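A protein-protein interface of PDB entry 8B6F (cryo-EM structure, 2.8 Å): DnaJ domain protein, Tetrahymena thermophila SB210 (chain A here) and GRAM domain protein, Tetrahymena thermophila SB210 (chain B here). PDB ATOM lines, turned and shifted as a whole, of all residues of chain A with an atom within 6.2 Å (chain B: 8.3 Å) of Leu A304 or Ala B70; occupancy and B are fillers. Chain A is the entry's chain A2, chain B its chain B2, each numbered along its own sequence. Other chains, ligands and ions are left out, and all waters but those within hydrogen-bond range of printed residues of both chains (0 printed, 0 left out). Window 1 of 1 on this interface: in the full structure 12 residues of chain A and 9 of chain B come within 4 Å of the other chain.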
ATOM      1  N   LEU A 273      29.456  18.718  23.465  1.00  0.00           N
ATOM      2  CA  LEU A 273      29.092  17.659  24.401  1.00  0.00           C
ATOM      3  C   LEU A 273      29.975  16.435  24.208  1.00  0.00           C
ATOM      4  O   LEU A 273      30.400  15.807  25.185  1.00  0.00           O
ATOM      5  CB  LEU A 273      27.618  17.291  24.232  1.00  0.00           C
ATOM      6  CG  LEU A 273      26.599  18.354  24.654  1.00  0.00           C
ATOM      7  CD1 LEU A 273      25.196  17.926  24.264  1.00  0.00           C
ATOM      8  CD2 LEU A 273      26.673  18.626  26.149  1.00  0.00           C
ATOM      9  N   SER A 274      30.255  16.071  22.957  1.00  0.00           N
ATOM     10  CA  SER A 274      31.113  14.919  22.701  1.00  0.00           C
ATOM     11  C   SER A 274      32.498  15.130  23.297  1.00  0.00           C
ATOM     12  O   SER A 274      33.032  14.252  23.984  1.00  0.00           O
ATOM     13  CB  SER A 274      31.211  14.667  21.196  1.00  0.00           C
ATOM     14  OG  SER A 274      29.926  14.536  20.615  1.00  0.00           O
ATOM     15  N   TYR A 277      32.405  15.052  27.191  1.00  0.00           N
ATOM     16  CA  TYR A 277      32.336  13.698  27.727  1.00  0.00           C
ATOM     17  C   TYR A 277      33.653  12.963  27.518  1.00  0.00           C
ATOM     18  O   TYR A 277      34.081  12.189  28.382  1.00  0.00           O
ATOM     19  CB  TYR A 277      31.187  12.927  27.082  1.00  0.00           C
ATOM     20  CG  TYR A 277      30.881  11.620  27.779  1.00  0.00           C
ATOM     21  CD1 TYR A 277      31.514  10.443  27.406  1.00  0.00           C
ATOM     22  CD2 TYR A 277      29.962  11.569  28.818  1.00  0.00           C
ATOM     23  CE1 TYR A 277      31.237   9.251  28.044  1.00  0.00           C
ATOM     24  CE2 TYR A 277      29.678  10.382  29.462  1.00  0.00           C
ATOM     25  CZ  TYR A 277      30.317   9.227  29.071  1.00  0.00           C
ATOM     26  OH  TYR A 277      30.034   8.044  29.713  1.00  0.00           O
ATOM     27  N   LYS A 278      34.307  13.189  26.378  1.00  0.00           N
ATOM     28  CA  LYS A 278      35.591  12.541  26.127  1.00  0.00           C
ATOM     29  C   LYS A 278      36.621  12.960  27.168  1.00  0.00           C
ATOM     30  O   LYS A 278      37.458  12.151  27.585  1.00  0.00           O
ATOM     31  CB  LYS A 278      36.077  12.875  24.717  1.00  0.00           C
ATOM     32  CG  LYS A 278      37.324  12.112  24.295  1.00  0.00           C
ATOM     33  CD  LYS A 278      37.687  12.406  22.847  1.00  0.00           C
ATOM     34  CE  LYS A 278      38.905  11.610  22.403  1.00  0.00           C
ATOM     35  NZ  LYS A 278      40.116  11.935  23.207  1.00  0.00           N
ATOM     36  N   VAL A 296      24.272  13.061  29.597  1.00  0.00           N
ATOM     37  CA  VAL A 296      24.992  12.400  28.515  1.00  0.00           C
ATOM     38  C   VAL A 296      25.525  11.081  29.056  1.00  0.00           C
ATOM     39  O   VAL A 296      26.369  11.068  29.960  1.00  0.00           O
ATOM     40  CB  VAL A 296      26.129  13.282  27.976  1.00  0.00           C
ATOM     41  CG1 VAL A 296      26.813  12.612  26.795  1.00  0.00           C
ATOM     42  CG2 VAL A 296      25.599  14.653  27.583  1.00  0.00           C
ATOM     43  N   THR A 297      25.034   9.972  28.510  1.00  0.00           N
ATOM     44  CA  THR A 297      25.366   8.644  29.005  1.00  0.00           C
ATOM     45  C   THR A 297      25.834   7.766  27.856  1.00  0.00           C
ATOM     46  O   THR A 297      25.362   7.894  26.724  1.00  0.00           O
ATOM     47  CB  THR A 297      24.162   7.987  29.701  1.00  0.00           C
ATOM     48  OG1 THR A 297      24.530   6.685  30.174  1.00  0.00           O
ATOM     49  CG2 THR A 297      22.984   7.860  28.745  1.00  0.00           C
ATOM     50  N   GLN A 298      26.769   6.870  28.159  1.00  0.00           N
ATOM     51  CA  GLN A 298      27.324   5.949  27.178  1.00  0.00           C
ATOM     52  C   GLN A 298      26.660   4.586  27.340  1.00  0.00           C
ATOM     53  O   GLN A 298      26.758   3.968  28.405  1.00  0.00           O
ATOM     54  CB  GLN A 298      28.839   5.828  27.334  1.00  0.00           C
ATOM     55  CG  GLN A 298      29.491   4.977  26.255  1.00  0.00           C
ATOM     56  CD  GLN A 298      30.994   5.138  26.217  1.00  0.00           C
ATOM     57  OE1 GLN A 298      31.506   6.243  26.047  1.00  0.00           O
ATOM     58  NE2 GLN A 298      31.711   4.034  26.380  1.00  0.00           N
ATOM     59  N   ARG A 299      25.995   4.124  26.286  1.00  0.00           N
ATOM     60  CA  ARG A 299      25.369   2.816  26.305  1.00  0.00           C
ATOM     61  C   ARG A 299      26.437   1.724  26.277  1.00  0.00           C
ATOM     62  O   ARG A 299      27.571   1.963  25.857  1.00  0.00           O
ATOM     63  CB  ARG A 299      24.426   2.671  25.115  1.00  0.00           C
ATOM     64  CG  ARG A 299      23.284   3.675  25.115  1.00  0.00           C
ATOM     65  CD  ARG A 299      22.314   3.425  26.259  1.00  0.00           C
ATOM     66  NE  ARG A 299      21.328   4.491  26.383  1.00  0.00           N
ATOM     67  CZ  ARG A 299      20.206   4.565  25.681  1.00  0.00           C
ATOM     68  NH1 ARG A 299      19.894   3.654  24.774  1.00  0.00           N
ATOM     69  NH2 ARG A 299      19.370   5.578  25.897  1.00  0.00           N
ATOM     70  N   ASN A 301      27.017  -0.636  24.312  1.00  0.00           N
ATOM     71  CA  ASN A 301      27.595  -0.801  22.986  1.00  0.00           C
ATOM     72  C   ASN A 301      28.545   0.331  22.616  1.00  0.00           C
ATOM     73  O   ASN A 301      29.228   0.230  21.592  1.00  0.00           O
ATOM     74  CB  ASN A 301      26.487  -0.913  21.937  1.00  0.00           C
ATOM     75  CG  ASN A 301      25.538   0.265  21.963  1.00  0.00           C
ATOM     76  OD1 ASN A 301      25.843   1.311  22.534  1.00  0.00           O
ATOM     77  ND2 ASN A 301      24.377   0.101  21.344  1.00  0.00           N
ATOM     78  N   GLY A 302      28.602   1.395  23.409  1.00  0.00           N
ATOM     79  CA  GLY A 302      29.502   2.498  23.151  1.00  0.00           C
ATOM     80  C   GLY A 302      28.888   3.695  22.458  1.00  0.00           C
ATOM     81  O   GLY A 302      29.635   4.520  21.921  1.00  0.00           O
ATOM     82  N   LEU A 303      27.563   3.819  22.454  1.00  0.00           N
ATOM     83  CA  LEU A 303      26.870   4.900  21.763  1.00  0.00           C
ATOM     84  C   LEU A 303      26.460   5.959  22.782  1.00  0.00           C
ATOM     85  O   LEU A 303      25.637   5.695  23.663  1.00  0.00           O
ATOM     86  CB  LEU A 303      25.655   4.353  21.015  1.00  0.00           C
ATOM     87  CG  LEU A 303      24.794   5.349  20.237  1.00  0.00           C
ATOM     88  CD1 LEU A 303      25.612   6.075  19.189  1.00  0.00           C
ATOM     89  CD2 LEU A 303      23.624   4.635  19.591  1.00  0.00           C
ATOM     90  N   LEU A 304      27.038   7.153  22.665  1.00  0.00           N
ATOM     91  CA  LEU A 304      26.658   8.255  23.540  1.00  0.00           C
ATOM     92  C   LEU A 304      25.268   8.761  23.181  1.00  0.00           C
ATOM     93  O   LEU A 304      24.928   8.915  22.006  1.00  0.00           O
ATOM     94  CB  LEU A 304      27.663   9.403  23.440  1.00  0.00           C
ATOM     95  CG  LEU A 304      29.084   9.172  23.958  1.00  0.00           C
ATOM     96  CD1 LEU A 304      29.854  10.483  23.982  1.00  0.00           C
ATOM     97  CD2 LEU A 304      29.082   8.537  25.336  1.00  0.00           C
ATOM     98  N   VAL A 305      24.465   9.029  24.207  1.00  0.00           N
ATOM     99  CA  VAL A 305      23.107   9.525  24.033  1.00  0.00           C
ATOM    100  C   VAL A 305      22.855  10.628  25.050  1.00  0.00           C
ATOM    101  O   VAL A 305      23.261  10.522  26.211  1.00  0.00           O
ATOM    102  CB  VAL A 305      22.065   8.397  24.178  1.00  0.00           C
ATOM    103  CG1 VAL A 305      22.309   7.317  23.144  1.00  0.00           C
ATOM    104  CG2 VAL A 305      22.102   7.808  25.578  1.00  0.00           C
ATOM    105  N   ALA A 306      22.190  11.689  24.606  1.00  0.00           N
ATOM    106  CA  ALA A 306      21.789  12.790  25.468  1.00  0.00           C
ATOM    107  C   ALA A 306      20.293  12.694  25.733  1.00  0.00           C
ATOM    108  O   ALA A 306      19.495  12.632  24.792  1.00  0.00           O
ATOM    109  CB  ALA A 306      22.129  14.137  24.830  1.00  0.00           C
ATOM    110  N   ARG B  67      18.799  13.177  20.210  1.00  0.00           N
ATOM    111  CA  ARG B  67      19.048  11.995  21.030  1.00  0.00           C
ATOM    112  C   ARG B  67      20.429  11.384  20.850  1.00  0.00           C
ATOM    113  O   ARG B  67      20.883  10.681  21.760  1.00  0.00           O
ATOM    114  CB  ARG B  67      17.997  10.917  20.745  1.00  0.00           C
ATOM    115  CG  ARG B  67      18.128   9.694  21.636  1.00  0.00           C
ATOM    116  CD  ARG B  67      16.939   8.768  21.489  1.00  0.00           C
ATOM    117  NE  ARG B  67      16.986   7.684  22.462  1.00  0.00           N
ATOM    118  CZ  ARG B  67      16.588   7.789  23.722  1.00  0.00           C
ATOM    119  NH1 ARG B  67      16.112   8.925  24.204  1.00  0.00           N
ATOM    120  NH2 ARG B  67      16.668   6.727  24.518  1.00  0.00           N
ATOM    121  N   ILE B  68      21.120  11.614  19.737  1.00  0.00           N
ATOM    122  CA  ILE B  68      22.401  10.980  19.448  1.00  0.00           C
ATOM    123  C   ILE B  68      23.481  12.050  19.474  1.00  0.00           C
ATOM    124  O   ILE B  68      23.328  13.110  18.854  1.00  0.00           O
ATOM    125  CB  ILE B  68      22.382  10.254  18.091  1.00  0.00           C
ATOM    126  CG1 ILE B  68      21.273   9.201  18.055  1.00  0.00           C
ATOM    127  CG2 ILE B  68      23.738   9.614  17.801  1.00  0.00           C
ATOM    128  CD1 ILE B  68      21.416   8.097  19.084  1.00  0.00           C
ATOM    129  N   VAL B  69      24.569  11.773  20.187  1.00  0.00           N
ATOM    130  CA  VAL B  69      25.691  12.697  20.316  1.00  0.00           C
ATOM    131  C   VAL B  69      26.906  12.201  19.537  1.00  0.00           C
ATOM    132  O   VAL B  69      27.418  12.898  18.658  1.00  0.00           O
ATOM    133  CB  VAL B  69      26.038  12.942  21.802  1.00  0.00           C
ATOM    134  CG1 VAL B  69      27.256  13.841  21.932  1.00  0.00           C
ATOM    135  CG2 VAL B  69      24.849  13.549  22.525  1.00  0.00           C
ATOM    136  N   ALA B  70      27.383  10.994  19.842  1.00  0.00           N
ATOM    137  CA  ALA B  70      28.574  10.458  19.196  1.00  0.00           C
ATOM    138  C   ALA B  70      28.436   8.953  19.029  1.00  0.00           C
ATOM    139  O   ALA B  70      28.156   8.243  19.999  1.00  0.00           O
ATOM    140  CB  ALA B  70      29.831  10.782  20.008  1.00  0.00           C
ATOM    141  N   LEU B  71      28.633   8.476  17.800  1.00  0.00           N
ATOM    142  CA  LEU B  71      28.639   7.048  17.525  1.00  0.00           C
ATOM    143  C   LEU B  71      30.012   6.451  17.827  1.00  0.00           C
ATOM    144  O   LEU B  71      31.024   7.154  17.788  1.00  0.00           O
ATOM    145  CB  LEU B  71      28.278   6.780  16.068  1.00  0.00           C
ATOM    146  CG  LEU B  71      26.820   6.972  15.644  1.00  0.00           C
ATOM    147  CD1 LEU B  71      26.385   8.418  15.767  1.00  0.00           C
ATOM    148  CD2 LEU B  71      26.633   6.481  14.222  1.00  0.00           C
ATOM    149  N   PRO B  72      30.074   5.155  18.128  1.00  0.00           N
ATOM    150  CA  PRO B  72      31.374   4.525  18.378  1.00  0.00           C
ATOM    151  C   PRO B  72      32.228   4.473  17.124  1.00  0.00           C
ATOM    152  O   PRO B  72      31.727   4.290  16.013  1.00  0.00           O
ATOM    153  CB  PRO B  72      31.002   3.118  18.856  1.00  0.00           C
ATOM    154  CG  PRO B  72      29.675   2.862  18.248  1.00  0.00           C
ATOM    155  CD  PRO B  72      28.969   4.185  18.214  1.00  0.00           C
ATOM    156  N   ARG B  73      33.534   4.632  17.313  1.00  0.00           N
ATOM    157  CA  ARG B  73      34.469   4.469  16.214  1.00  0.00           C
ATOM    158  C   ARG B  73      34.611   2.996  15.849  1.00  0.00           C
ATOM    159  O   ARG B  73      34.385   2.098  16.664  1.00  0.00           O
ATOM    160  CB  ARG B  73      35.833   5.054  16.578  1.00  0.00           C
ATOM    161  CG  ARG B  73      35.896   6.550  16.406  1.00  0.00           C
ATOM    162  CD  ARG B  73      36.065   6.895  14.941  1.00  0.00           C
ATOM    163  NE  ARG B  73      35.753   8.292  14.684  1.00  0.00           N
ATOM    164  CZ  ARG B  73      34.552   8.743  14.349  1.00  0.00           C
ATOM    165  NH1 ARG B  73      33.514   7.934  14.224  1.00  0.00           N
ATOM    166  NH2 ARG B  73      34.388  10.042  14.140  1.00  0.00           N
ATOM    167  N   VAL B  82      34.789   0.568  19.017  1.00  0.00           N
ATOM    168  CA  VAL B  82      35.333   1.124  20.252  1.00  0.00           C
ATOM    169  C   VAL B  82      34.550   2.395  20.564  1.00  0.00           C
ATOM    170  O   VAL B  82      34.199   3.139  19.638  1.00  0.00           O
ATOM    171  CB  VAL B  82      36.840   1.396  20.113  1.00  0.00           C
ATOM    172  CG1 VAL B  82      37.104   2.422  19.019  1.00  0.00           C
ATOM    173  CG2 VAL B  82      37.436   1.849  21.431  1.00  0.00           C
ATOM    174  N   PRO B  83      34.239   2.684  21.829  1.00  0.00           N
ATOM    175  CA  PRO B  83      33.482   3.904  22.127  1.00  0.00           C
ATOM    176  C   PRO B  83      34.230   5.153  21.686  1.00  0.00           C
ATOM    177  O   PRO B  83      35.461   5.211  21.709  1.00  0.00           O
ATOM    178  CB  PRO B  83      33.313   3.859  23.652  1.00  0.00           C
ATOM    179  CG  PRO B  83      34.342   2.896  24.133  1.00  0.00           C
ATOM    180  CD  PRO B  83      34.487   1.890  23.043  1.00  0.00           C
ATOM    181  N   PHE B  84      33.459   6.162  21.274  1.00  0.00           N
ATOM    182  CA  PHE B  84      34.052   7.421  20.837  1.00  0.00           C
ATOM    183  C   PHE B  84      34.896   8.050  21.934  1.00  0.00           C
ATOM    184  O   PHE B  84      35.854   8.775  21.642  1.00  0.00           O
ATOM    185  CB  PHE B  84      32.952   8.386  20.396  1.00  0.00           C
ATOM    186  CG  PHE B  84      33.467   9.681  19.833  1.00  0.00           C
ATOM    187  CD1 PHE B  84      33.785  10.740  20.667  1.00  0.00           C
ATOM    188  CD2 PHE B  84      33.616   9.844  18.466  1.00  0.00           C
ATOM    189  CE1 PHE B  84      34.254  11.933  20.150  1.00  0.00           C
ATOM    190  CE2 PHE B  84      34.083  11.033  17.942  1.00  0.00           C
ATOM    191  CZ  PHE B  84      34.402  12.079  18.785  1.00  0.00           C
ATOM    192  N   SER B  85      34.558   7.792  23.197  1.00  0.00           N
ATOM    193  CA  SER B  85      35.314   8.376  24.298  1.00  0.00           C
ATOM    194  C   SER B  85      36.759   7.892  24.294  1.00  0.00           C
ATOM    195  O   SER B  85      37.684   8.675  24.537  1.00  0.00           O
ATOM    196  CB  SER B  85      34.635   8.039  25.624  1.00  0.00           C
ATOM    197  OG  SER B  85      34.576   6.637  25.827  1.00  0.00           O
ATOM    198  N   GLN B  86      36.974   6.607  24.026  1.00  0.00           N
ATOM    199  CA  GLN B  86      38.325   6.060  24.011  1.00  0.00           C
ATOM    200  C   GLN B  86      39.143   6.679  22.885  1.00  0.00           C
ATOM    201  O   GLN B  86      38.639   6.913  21.784  1.00  0.00           O
ATOM    202  CB  GLN B  86      38.282   4.541  23.853  1.00  0.00           C
ATOM    203  CG  GLN B  86      39.657   3.893  23.776  1.00  0.00           C
ATOM    204  CD  GLN B  86      39.587   2.381  23.743  1.00  0.00           C
ATOM    205  OE1 GLN B  86      38.582   1.787  24.128  1.00  0.00           O
ATOM    206  NE2 GLN B  86      40.657   1.749  23.273  1.00  0.00           N
ATOM    207  N   HIS B  91      41.947   7.951  15.370  1.00  0.00           N
ATOM    208  CA  HIS B  91      40.899   8.909  15.691  1.00  0.00           C
ATOM    209  C   HIS B  91      41.168  10.241  15.002  1.00  0.00           C
ATOM    210  O   HIS B  91      42.315  10.680  14.885  1.00  0.00           O
ATOM    211  CB  HIS B  91      40.813   9.104  17.206  1.00  0.00           C
ATOM    212  CG  HIS B  91      39.488   9.621  17.676  1.00  0.00           C
ATOM    213  ND1 HIS B  91      39.224  10.964  17.832  1.00  0.00           N
ATOM    214  CD2 HIS B  91      38.353   8.972  18.026  1.00  0.00           C
ATOM    215  CE1 HIS B  91      37.983  11.120  18.257  1.00  0.00           C
ATOM    216  NE2 HIS B  91      37.432   9.927  18.383  1.00  0.00           N
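The backbone carbonyl oxygen (O) of Arg B67 sits at hydrogen-bond distance from the backbone NH (N) of Ala A306, 3.3 Å away.
The guanidinium group (NH2) of Arg B67 sits close to the guanidinium group (NH2) of Arg A299 (3.2 Å).
The backbone carbonyl oxygen (O) of Ala B70 is in hydrogen-bond range of the backbone NH (N) of Leu A304 (3.1 Å).
OE1 of Gln A298 sits at hydrogen-bond distance from OG of Ser B85, 3.1 Å away.
N of Val B69 sits at hydrogen-bond distance from O of Leu A304 (3.4 Å).
Of chain B, only Val B69 (3.4 Å) and Ala B70 (3.1 Å) come within 4 Å of Leu A304.
Of chain B, only Arg B67 (3.4 Å) comes within 4 Å of Val A305.
Printed residues of chain A within 4 Å of Arg B67: Arg A299 (3.2 Å), Val A305 (3.4 Å) and Ala A306 (3.3 Å).
Ala B70 touches three residues of chain A.
Of the printed residues of chain A, Pro B72 touches Gly A302 (3.6 Å) and Leu A303 (3.97 Å).
The nearest residue of chain B that does not touch Leu A304 is Ile B68 (4.1 Å).
O of Thr A297 is in hydrogen-bond range of N of Val A305, at 2.9 Å.
OD1 of Asn A301 lies within hydrogen-bond range of N of Leu A303 (3.0 Å).
Hydrophobic or aromatic side chains of chain A within 4 Å of the printed part of chain B: Leu A303, Leu A304, Val A305 and Ala A306.
Hydrophobic or aromatic side chains of chain B within 4 Å of the printed part of chain A: Val B69, Ala B70, Leu B71, Pro B72 and Pro B83.
Among the printed residues, 16 pairs touch across the chains.
Among the printed residues, no Asp or Glu carboxylate lies within 4 Å of a Lys or Arg side-chain nitrogen of the other chain.
Ala B70 touches Ser A274 (CB to OG, 3.8 Å).
Lys A278 touches Ser B85 (CG to O, 3.5 Å).
NE2 of Gln A298 touches CB of Pro B83 (3.2 Å).
CB of Pro B72 touches O of Gly A302, at 3.6 Å.
O of Gly A302 touches CA of Pro B83 (3.9 Å).
Ala B70 touches Leu A303.
CD1 of Leu A303 touches CA of Leu B71, 3.6 Å away.
Leu A303 touches Pro B72.
CA of Val A305 touches O of Arg B67, 3.4 Å away.
CG2 of Val B69 touches CB of Ala A306 (3.6 Å).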
